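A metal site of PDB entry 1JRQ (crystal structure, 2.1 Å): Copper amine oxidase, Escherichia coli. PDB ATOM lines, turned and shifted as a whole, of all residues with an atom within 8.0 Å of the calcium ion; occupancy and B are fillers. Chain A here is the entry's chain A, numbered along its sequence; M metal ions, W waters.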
ATOM      1  N   LYS A 133       3.071 -19.819  16.577  1.00  0.00           N
ATOM      2  CA  LYS A 133       2.520 -18.600  17.169  1.00  0.00           C
ATOM      3  C   LYS A 133       1.114 -18.299  16.647  1.00  0.00           C
ATOM      4  O   LYS A 133       0.208 -17.998  17.419  1.00  0.00           O
ATOM      5  CB  LYS A 133       3.486 -17.456  16.899  1.00  0.00           C
ATOM      6  CG  LYS A 133       2.981 -16.052  17.173  1.00  0.00           C
ATOM      7  CD  LYS A 133       4.105 -15.020  17.097  1.00  0.00           C
ATOM      8  CE  LYS A 133       3.643 -13.606  17.375  1.00  0.00           C
ATOM      9  NZ  LYS A 133       4.811 -12.741  17.724  1.00  0.00           N
ATOM     10  N   TRP A 137      -2.199 -17.986  19.130  1.00  0.00           N
ATOM     11  CA  TRP A 137      -3.026 -16.789  19.243  1.00  0.00           C
ATOM     12  C   TRP A 137      -4.482 -17.074  18.885  1.00  0.00           C
ATOM     13  O   TRP A 137      -5.351 -16.499  19.527  1.00  0.00           O
ATOM     14  CB  TRP A 137      -2.556 -15.642  18.345  1.00  0.00           C
ATOM     15  CG  TRP A 137      -1.645 -14.609  18.947  1.00  0.00           C
ATOM     16  CD1 TRP A 137      -0.468 -14.151  18.465  1.00  0.00           C
ATOM     17  CD2 TRP A 137      -1.877 -13.887  20.170  1.00  0.00           C
ATOM     18  NE1 TRP A 137       0.065 -13.184  19.294  1.00  0.00           N
ATOM     19  CE2 TRP A 137      -0.798 -13.017  20.354  1.00  0.00           C
ATOM     20  CE3 TRP A 137      -2.912 -13.906  21.116  1.00  0.00           C
ATOM     21  CZ2 TRP A 137      -0.707 -12.172  21.464  1.00  0.00           C
ATOM     22  CZ3 TRP A 137      -2.847 -13.075  22.211  1.00  0.00           C
ATOM     23  CH2 TRP A 137      -1.748 -12.226  22.360  1.00  0.00           C
ATOM     24  N   VAL A 356      -1.274  -7.687  23.109  1.00  0.00           N
ATOM     25  CA  VAL A 356      -0.283  -6.810  23.719  1.00  0.00           C
ATOM     26  C   VAL A 356       1.049  -7.547  23.621  1.00  0.00           C
ATOM     27  O   VAL A 356       2.000  -7.014  23.057  1.00  0.00           O
ATOM     28  CB  VAL A 356      -0.574  -6.384  25.173  1.00  0.00           C
ATOM     29  CG1 VAL A 356       0.588  -5.641  25.806  1.00  0.00           C
ATOM     30  CG2 VAL A 356      -1.863  -5.570  25.216  1.00  0.00           C
ATOM     31  N   MET A 357       1.080  -8.766  24.157  1.00  0.00           N
ATOM     32  CA  MET A 357       2.320  -9.540  24.101  1.00  0.00           C
ATOM     33  C   MET A 357       2.149 -11.037  23.904  1.00  0.00           C
ATOM     34  O   MET A 357       1.432 -11.737  24.632  1.00  0.00           O
ATOM     35  CB  MET A 357       3.125  -9.251  25.377  1.00  0.00           C
ATOM     36  CG  MET A 357       4.508  -9.892  25.393  1.00  0.00           C
ATOM     37  SD  MET A 357       5.525  -9.432  26.808  1.00  0.00           S
ATOM     38  CE  MET A 357       4.653 -10.195  28.174  1.00  0.00           C
ATOM     39  N   TYR A 358       2.840 -11.564  22.883  1.00  0.00           N
ATOM     40  CA  TYR A 358       2.758 -12.992  22.611  1.00  0.00           C
ATOM     41  C   TYR A 358       3.461 -13.790  23.703  1.00  0.00           C
ATOM     42  O   TYR A 358       2.900 -14.716  24.286  1.00  0.00           O
ATOM     43  CB  TYR A 358       3.301 -13.370  21.236  1.00  0.00           C
ATOM     44  CG  TYR A 358       3.158 -14.876  21.046  1.00  0.00           C
ATOM     45  CD1 TYR A 358       1.901 -15.467  21.047  1.00  0.00           C
ATOM     46  CD2 TYR A 358       4.279 -15.670  20.880  1.00  0.00           C
ATOM     47  CE1 TYR A 358       1.780 -16.841  20.880  1.00  0.00           C
ATOM     48  CE2 TYR A 358       4.178 -17.041  20.723  1.00  0.00           C
ATOM     49  CZ  TYR A 358       2.922 -17.613  20.718  1.00  0.00           C
ATOM     50  OH  TYR A 358       2.815 -18.977  20.550  1.00  0.00           O
ATOM     51  N   GLU A 359       4.710 -13.451  24.010  1.00  0.00           N
ATOM     52  CA  GLU A 359       5.464 -14.165  25.040  1.00  0.00           C
ATOM     53  C   GLU A 359       6.502 -13.196  25.614  1.00  0.00           C
ATOM     54  O   GLU A 359       7.112 -12.425  24.869  1.00  0.00           O
ATOM     55  CB  GLU A 359       6.294 -15.327  24.490  1.00  0.00           C
ATOM     56  CG  GLU A 359       5.575 -16.454  23.769  1.00  0.00           C
ATOM     57  CD  GLU A 359       6.535 -17.526  23.288  1.00  0.00           C
ATOM     58  OE1 GLU A 359       6.614 -18.603  23.916  1.00  0.00           O
ATOM     59  OE2 GLU A 359       7.236 -17.376  22.262  1.00  0.00           O
ATOM     60  N   ARG A 531      13.311 -10.683  27.147  1.00  0.00           N
ATOM     61  CA  ARG A 531      12.878 -10.950  25.774  1.00  0.00           C
ATOM     62  C   ARG A 531      11.364 -10.758  25.778  1.00  0.00           C
ATOM     63  O   ARG A 531      10.616 -11.532  26.396  1.00  0.00           O
ATOM     64  CB  ARG A 531      13.271 -12.348  25.301  1.00  0.00           C
ATOM     65  CG  ARG A 531      12.680 -12.708  23.947  1.00  0.00           C
ATOM     66  CD  ARG A 531      13.017 -14.135  23.511  1.00  0.00           C
ATOM     67  NE  ARG A 531      12.415 -14.456  22.218  1.00  0.00           N
ATOM     68  CZ  ARG A 531      11.131 -14.646  21.986  1.00  0.00           C
ATOM     69  NH1 ARG A 531      10.264 -14.547  22.991  1.00  0.00           N
ATOM     70  NH2 ARG A 531      10.667 -14.917  20.767  1.00  0.00           N
ATOM     71  N   LEU A 532      10.921  -9.707  25.100  1.00  0.00           N
ATOM     72  CA  LEU A 532       9.514  -9.364  24.992  1.00  0.00           C
ATOM     73  C   LEU A 532       8.947  -9.356  23.581  1.00  0.00           C
ATOM     74  O   LEU A 532       9.040  -8.419  22.784  1.00  0.00           O
ATOM     75  CB  LEU A 532       9.317  -7.999  25.686  1.00  0.00           C
ATOM     76  CG  LEU A 532      10.082  -7.862  27.010  1.00  0.00           C
ATOM     77  CD1 LEU A 532      10.152  -6.413  27.490  1.00  0.00           C
ATOM     78  CD2 LEU A 532       9.413  -8.727  28.095  1.00  0.00           C
ATOM     79  N   ASP A 533       8.291 -10.476  23.235  1.00  0.00           N
ATOM     80  CA  ASP A 533       7.692 -10.569  21.901  1.00  0.00           C
ATOM     81  C   ASP A 533       6.368  -9.806  21.948  1.00  0.00           C
ATOM     82  O   ASP A 533       5.270 -10.349  21.982  1.00  0.00           O
ATOM     83  CB  ASP A 533       7.528 -12.023  21.468  1.00  0.00           C
ATOM     84  CG  ASP A 533       6.846 -12.159  20.120  1.00  0.00           C
ATOM     85  OD1 ASP A 533       6.799 -11.167  19.389  1.00  0.00           O
ATOM     86  OD2 ASP A 533       6.327 -13.217  19.717  1.00  0.00           O
ATOM     87  N   LEU A 534       6.475  -8.477  21.931  1.00  0.00           N
ATOM     88  CA  LEU A 534       5.302  -7.627  21.967  1.00  0.00           C
ATOM     89  C   LEU A 534       4.598  -7.691  20.616  1.00  0.00           C
ATOM     90  O   LEU A 534       5.343  -7.671  19.645  1.00  0.00           O
ATOM     91  CB  LEU A 534       5.706  -6.151  22.186  1.00  0.00           C
ATOM     92  CG  LEU A 534       6.309  -5.886  23.572  1.00  0.00           C
ATOM     93  CD1 LEU A 534       6.841  -4.457  23.616  1.00  0.00           C
ATOM     94  CD2 LEU A 534       5.277  -6.163  24.665  1.00  0.00           C
ATOM     95  N   ASP A 535       3.291  -7.744  20.556  1.00  0.00           N
ATOM     96  CA  ASP A 535       2.517  -7.789  19.330  1.00  0.00           C
ATOM     97  C   ASP A 535       1.533  -6.637  19.626  1.00  0.00           C
ATOM     98  O   ASP A 535       0.436  -6.872  20.127  1.00  0.00           O
ATOM     99  CB  ASP A 535       1.757  -9.079  19.071  1.00  0.00           C
ATOM    100  CG  ASP A 535       2.607 -10.252  18.625  1.00  0.00           C
ATOM    101  OD1 ASP A 535       3.770 -10.116  18.218  1.00  0.00           O
ATOM    102  OD2 ASP A 535       2.129 -11.400  18.654  1.00  0.00           O
ATOM    103  N   VAL A 536       1.944  -5.411  19.331  1.00  0.00           N
ATOM    104  CA  VAL A 536       1.056  -4.286  19.613  1.00  0.00           C
ATOM    105  C   VAL A 536      -0.229  -4.272  18.810  1.00  0.00           C
ATOM    106  O   VAL A 536      -0.200  -3.807  17.654  1.00  0.00           O
ATOM    107  CB  VAL A 536       1.800  -2.939  19.507  1.00  0.00           C
ATOM    108  CG1 VAL A 536       0.854  -1.787  19.839  1.00  0.00           C
ATOM    109  CG2 VAL A 536       3.019  -2.952  20.412  1.00  0.00           C
ATOM    110  N   GLY A 538      -1.506  -6.426  17.334  1.00  0.00           N
ATOM    111  CA  GLY A 538      -1.361  -7.164  16.080  1.00  0.00           C
ATOM    112  C   GLY A 538       0.103  -7.560  15.914  1.00  0.00           C
ATOM    113  O   GLY A 538       0.969  -7.074  16.638  1.00  0.00           O
ATOM    114  N   GLU A 539       0.347  -8.441  14.958  1.00  0.00           N
ATOM    115  CA  GLU A 539       1.696  -8.912  14.670  1.00  0.00           C
ATOM    116  C   GLU A 539       2.636  -7.899  14.032  1.00  0.00           C
ATOM    117  O   GLU A 539       3.771  -7.643  14.436  1.00  0.00           O
ATOM    118  CB  GLU A 539       1.549 -10.037  13.629  1.00  0.00           C
ATOM    119  CG  GLU A 539       2.852 -10.749  13.302  1.00  0.00           C
ATOM    120  CD  GLU A 539       2.724 -11.792  12.224  1.00  0.00           C
ATOM    121  OE1 GLU A 539       2.081 -12.841  12.427  1.00  0.00           O
ATOM    122  OE2 GLU A 539       3.238 -11.642  11.109  1.00  0.00           O
ATOM    123  N   ASN A 540       2.169  -7.268  12.962  1.00  0.00           N
ATOM    124  CA  ASN A 540       2.960  -6.290  12.228  1.00  0.00           C
ATOM    125  C   ASN A 540       3.130  -4.923  12.861  1.00  0.00           C
ATOM    126  O   ASN A 540       2.184  -4.148  12.913  1.00  0.00           O
ATOM    127  CB  ASN A 540       2.408  -6.215  10.799  1.00  0.00           C
ATOM    128  CG  ASN A 540       2.412  -7.591  10.152  1.00  0.00           C
ATOM    129  OD1 ASN A 540       3.345  -8.382  10.321  1.00  0.00           O
ATOM    130  ND2 ASN A 540       1.376  -7.944   9.404  1.00  0.00           N
ATOM    131  N   ASN A 541       4.330  -4.633  13.348  1.00  0.00           N
ATOM    132  CA  ASN A 541       4.629  -3.362  13.987  1.00  0.00           C
ATOM    133  C   ASN A 541       5.913  -2.748  13.444  1.00  0.00           C
ATOM    134  O   ASN A 541       6.636  -3.347  12.637  1.00  0.00           O
ATOM    135  CB  ASN A 541       4.828  -3.591  15.496  1.00  0.00           C
ATOM    136  CG  ASN A 541       3.716  -4.351  16.194  1.00  0.00           C
ATOM    137  OD1 ASN A 541       2.532  -4.297  15.843  1.00  0.00           O
ATOM    138  ND2 ASN A 541       4.112  -5.093  17.233  1.00  0.00           N
ATOM    139  N   LEU A 588       6.937   1.033  19.934  1.00  0.00           N
ATOM    140  CA  LEU A 588       6.748  -0.157  19.123  1.00  0.00           C
ATOM    141  C   LEU A 588       5.320   0.194  18.695  1.00  0.00           C
ATOM    142  O   LEU A 588       4.386   0.120  19.503  1.00  0.00           O
ATOM    143  CB  LEU A 588       6.898  -1.527  19.792  1.00  0.00           C
ATOM    144  CG  LEU A 588       6.685  -2.685  18.811  1.00  0.00           C
ATOM    145  CD1 LEU A 588       7.736  -2.610  17.708  1.00  0.00           C
ATOM    146  CD2 LEU A 588       6.711  -4.061  19.447  1.00  0.00           C
ATOM    147  N   VAL A 640      15.799  -4.942  18.924  1.00  0.00           N
ATOM    148  CA  VAL A 640      14.535  -5.313  18.303  1.00  0.00           C
ATOM    149  C   VAL A 640      14.959  -6.236  17.158  1.00  0.00           C
ATOM    150  O   VAL A 640      15.839  -5.848  16.380  1.00  0.00           O
ATOM    151  CB  VAL A 640      13.657  -4.168  17.787  1.00  0.00           C
ATOM    152  CG1 VAL A 640      12.340  -4.690  17.248  1.00  0.00           C
ATOM    153  CG2 VAL A 640      13.405  -3.123  18.870  1.00  0.00           C
ATOM    154  N   THR A 641      14.357  -7.424  17.073  1.00  0.00           N
ATOM    155  CA  THR A 641      14.757  -8.327  15.993  1.00  0.00           C
ATOM    156  C   THR A 641      13.478  -8.897  15.400  1.00  0.00           C
ATOM    157  O   THR A 641      12.427  -8.692  16.013  1.00  0.00           O
ATOM    158  CB  THR A 641      15.583  -9.518  16.522  1.00  0.00           C
ATOM    159  OG1 THR A 641      14.782 -10.251  17.478  1.00  0.00           O
ATOM    160  CG2 THR A 641      16.838  -9.036  17.235  1.00  0.00           C
ATOM    161  N   ARG A 642      13.632  -9.570  14.262  1.00  0.00           N
ATOM    162  CA  ARG A 642      12.472 -10.174  13.601  1.00  0.00           C
ATOM    163  C   ARG A 642      12.109 -11.422  14.419  1.00  0.00           C
ATOM    164  O   ARG A 642      13.052 -12.088  14.828  1.00  0.00           O
ATOM    165  CB  ARG A 642      12.849 -10.641  12.196  1.00  0.00           C
ATOM    166  CG  ARG A 642      13.158  -9.534  11.188  1.00  0.00           C
ATOM    167  CD  ARG A 642      12.679 -10.016   9.822  1.00  0.00           C
ATOM    168  NE  ARG A 642      12.100  -8.928   9.043  1.00  0.00           N
ATOM    169  CZ  ARG A 642      11.224  -9.112   8.074  1.00  0.00           C
ATOM    170  NH1 ARG A 642      10.838 -10.353   7.802  1.00  0.00           N
ATOM    171  NH2 ARG A 642      10.769  -8.050   7.428  1.00  0.00           N
ATOM    172  N   TYR A 643      10.823 -11.669  14.617  1.00  0.00           N
ATOM    173  CA  TYR A 643      10.389 -12.838  15.377  1.00  0.00           C
ATOM    174  C   TYR A 643      10.940 -14.110  14.748  1.00  0.00           C
ATOM    175  O   TYR A 643      10.787 -14.270  13.546  1.00  0.00           O
ATOM    176  CB  TYR A 643       8.854 -12.944  15.364  1.00  0.00           C
ATOM    177  CG  TYR A 643       8.391 -14.267  15.919  1.00  0.00           C
ATOM    178  CD1 TYR A 643       8.543 -14.552  17.274  1.00  0.00           C
ATOM    179  CD2 TYR A 643       7.819 -15.238  15.107  1.00  0.00           C
ATOM    180  CE1 TYR A 643       8.144 -15.758  17.811  1.00  0.00           C
ATOM    181  CE2 TYR A 643       7.412 -16.451  15.653  1.00  0.00           C
ATOM    182  CZ  TYR A 643       7.579 -16.698  16.998  1.00  0.00           C
ATOM    183  OH  TYR A 643       7.181 -17.903  17.536  1.00  0.00           O
ATOM    184  N   THR A 677       6.554  -5.428  10.516  1.00  0.00           N
ATOM    185  CA  THR A 677       6.712  -6.895  10.587  1.00  0.00           C
ATOM    186  C   THR A 677       6.682  -7.358  12.027  1.00  0.00           C
ATOM    187  O   THR A 677       6.646  -6.526  12.941  1.00  0.00           O
ATOM    188  CB  THR A 677       8.027  -7.216   9.858  1.00  0.00           C
ATOM    189  OG1 THR A 677       8.081  -8.600   9.535  1.00  0.00           O
ATOM    190  CG2 THR A 677       9.228  -6.780  10.689  1.00  0.00           C
ATOM    191  N   ASP A 678       6.675  -8.664  12.269  1.00  0.00           N
ATOM    192  CA  ASP A 678       6.639  -9.206  13.620  1.00  0.00           C
ATOM    193  C   ASP A 678       7.934  -8.922  14.370  1.00  0.00           C
ATOM    194  O   ASP A 678       8.948  -9.584  14.146  1.00  0.00           O
ATOM    195  CB  ASP A 678       6.337 -10.705  13.574  1.00  0.00           C
ATOM    196  CG  ASP A 678       6.000 -11.278  14.931  1.00  0.00           C
ATOM    197  OD1 ASP A 678       6.340 -10.630  15.932  1.00  0.00           O
ATOM    198  OD2 ASP A 678       5.410 -12.380  15.031  1.00  0.00           O
ATOM    199  N   ALA A 679       7.968  -7.948  15.282  1.00  0.00           N
ATOM    200  CA  ALA A 679       9.170  -7.612  16.024  1.00  0.00           C
ATOM    201  C   ALA A 679       9.249  -8.226  17.423  1.00  0.00           C
ATOM    202  O   ALA A 679       8.236  -8.535  18.035  1.00  0.00           O
ATOM    203  CB  ALA A 679       9.246  -6.106  16.278  1.00  0.00           C
ATOM    204  N   VAL A 680      10.463  -8.392  17.924  1.00  0.00           N
ATOM    205  CA  VAL A 680      10.673  -8.946  19.258  1.00  0.00           C
ATOM    206  C   VAL A 680      11.583  -7.936  19.956  1.00  0.00           C
ATOM    207  O   VAL A 680      12.670  -7.687  19.433  1.00  0.00           O
ATOM    208  CB  VAL A 680      11.318 -10.340  19.273  1.00  0.00           C
ATOM    209  CG1 VAL A 680      11.462 -10.841  20.707  1.00  0.00           C
ATOM    210  CG2 VAL A 680      10.455 -11.333  18.496  1.00  0.00           C
ATOM    211  N   VAL A 681      11.155  -7.386  21.080  1.00  0.00           N
ATOM    212  CA  VAL A 681      11.946  -6.404  21.812  1.00  0.00           C
ATOM    213  C   VAL A 681      12.783  -7.040  22.898  1.00  0.00           C
ATOM    214  O   VAL A 681      12.297  -7.934  23.595  1.00  0.00           O
ATOM    215  CB  VAL A 681      11.018  -5.357  22.456  1.00  0.00           C
ATOM    216  CG1 VAL A 681      11.787  -4.381  23.336  1.00  0.00           C
ATOM    217  CG2 VAL A 681      10.244  -4.607  21.367  1.00  0.00           C
HETATM  218 CA    CA M   1       6.019  -9.373  17.986  1.00  0.00          CA
HETATM  219  O   HOH W   1       5.235  -7.334  16.531  1.00  0.00           O
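Water W1 lies within hydrogen-bond range of the backbone carbonyl oxygen of Glu 539 (2.6 Å), the side-chain amide nitrogen of Asn 541 (2.6 Å) and the backbone NH of Ala 679 (3.1 Å).
NZ of Lys 133 touches the calcium ion, at 3.6 Å.
Six residues have an atom within 4 Å of the calcium ion: Lys 133, Asp 533, Leu 534, Asp 535, Asp 678 and Ala 679.
The nearest printed residue that does not touch the calcium ion is Glu 539 (4.5 Å).
The side-chain amino group (NZ) of Lys 133 is in salt-bridge range of the side-chain carboxylate (OD2) of Asp 535 (3.1 Å).
The backbone NH (N) of Asp 535 sits at hydrogen-bond distance from the backbone carbonyl oxygen (O) of Val 356 (2.9 Å).
The side-chain carboxylate (OD2) of Asp 535 lies within hydrogen-bond range of the indole nitrogen (NE1) of Trp 137 (2.8 Å).
The side-chain carboxylate (OD2) of Asp 533 is in salt-bridge range of the side-chain amino group (NZ) of Lys 133 (2.5 Å).
O of Asp 533 sits at hydrogen-bond distance from N of Tyr 358 (2.9 Å).
The backbone NH of Asp 533 sits at hydrogen-bond distance from the backbone carbonyl oxygen of Glu 359 (2.8 Å).
OD2 of Asp 678 lies within salt-bridge range of NZ of Lys 133, 2.8 Å away.
The backbone carbonyl oxygen (O) of Asp 678 lies within hydrogen-bond range of the backbone NH (N) of Tyr 643, at 2.8 Å.
The calcium ion is bound by the backbone carbonyl oxygen (O) of Ala 679 (2.4 Å), the side-chain carboxylate (OD1) of Asp 535 (2.4 Å), the side-chain carboxylate (OD1) of Asp 533 (2.4 Å), the side-chain carboxylate (OD1) of Asp 678 (2.4 Å), the backbone carbonyl oxygen (O) of Leu 534 (2.5 Å) and water W1 (2.6 Å).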
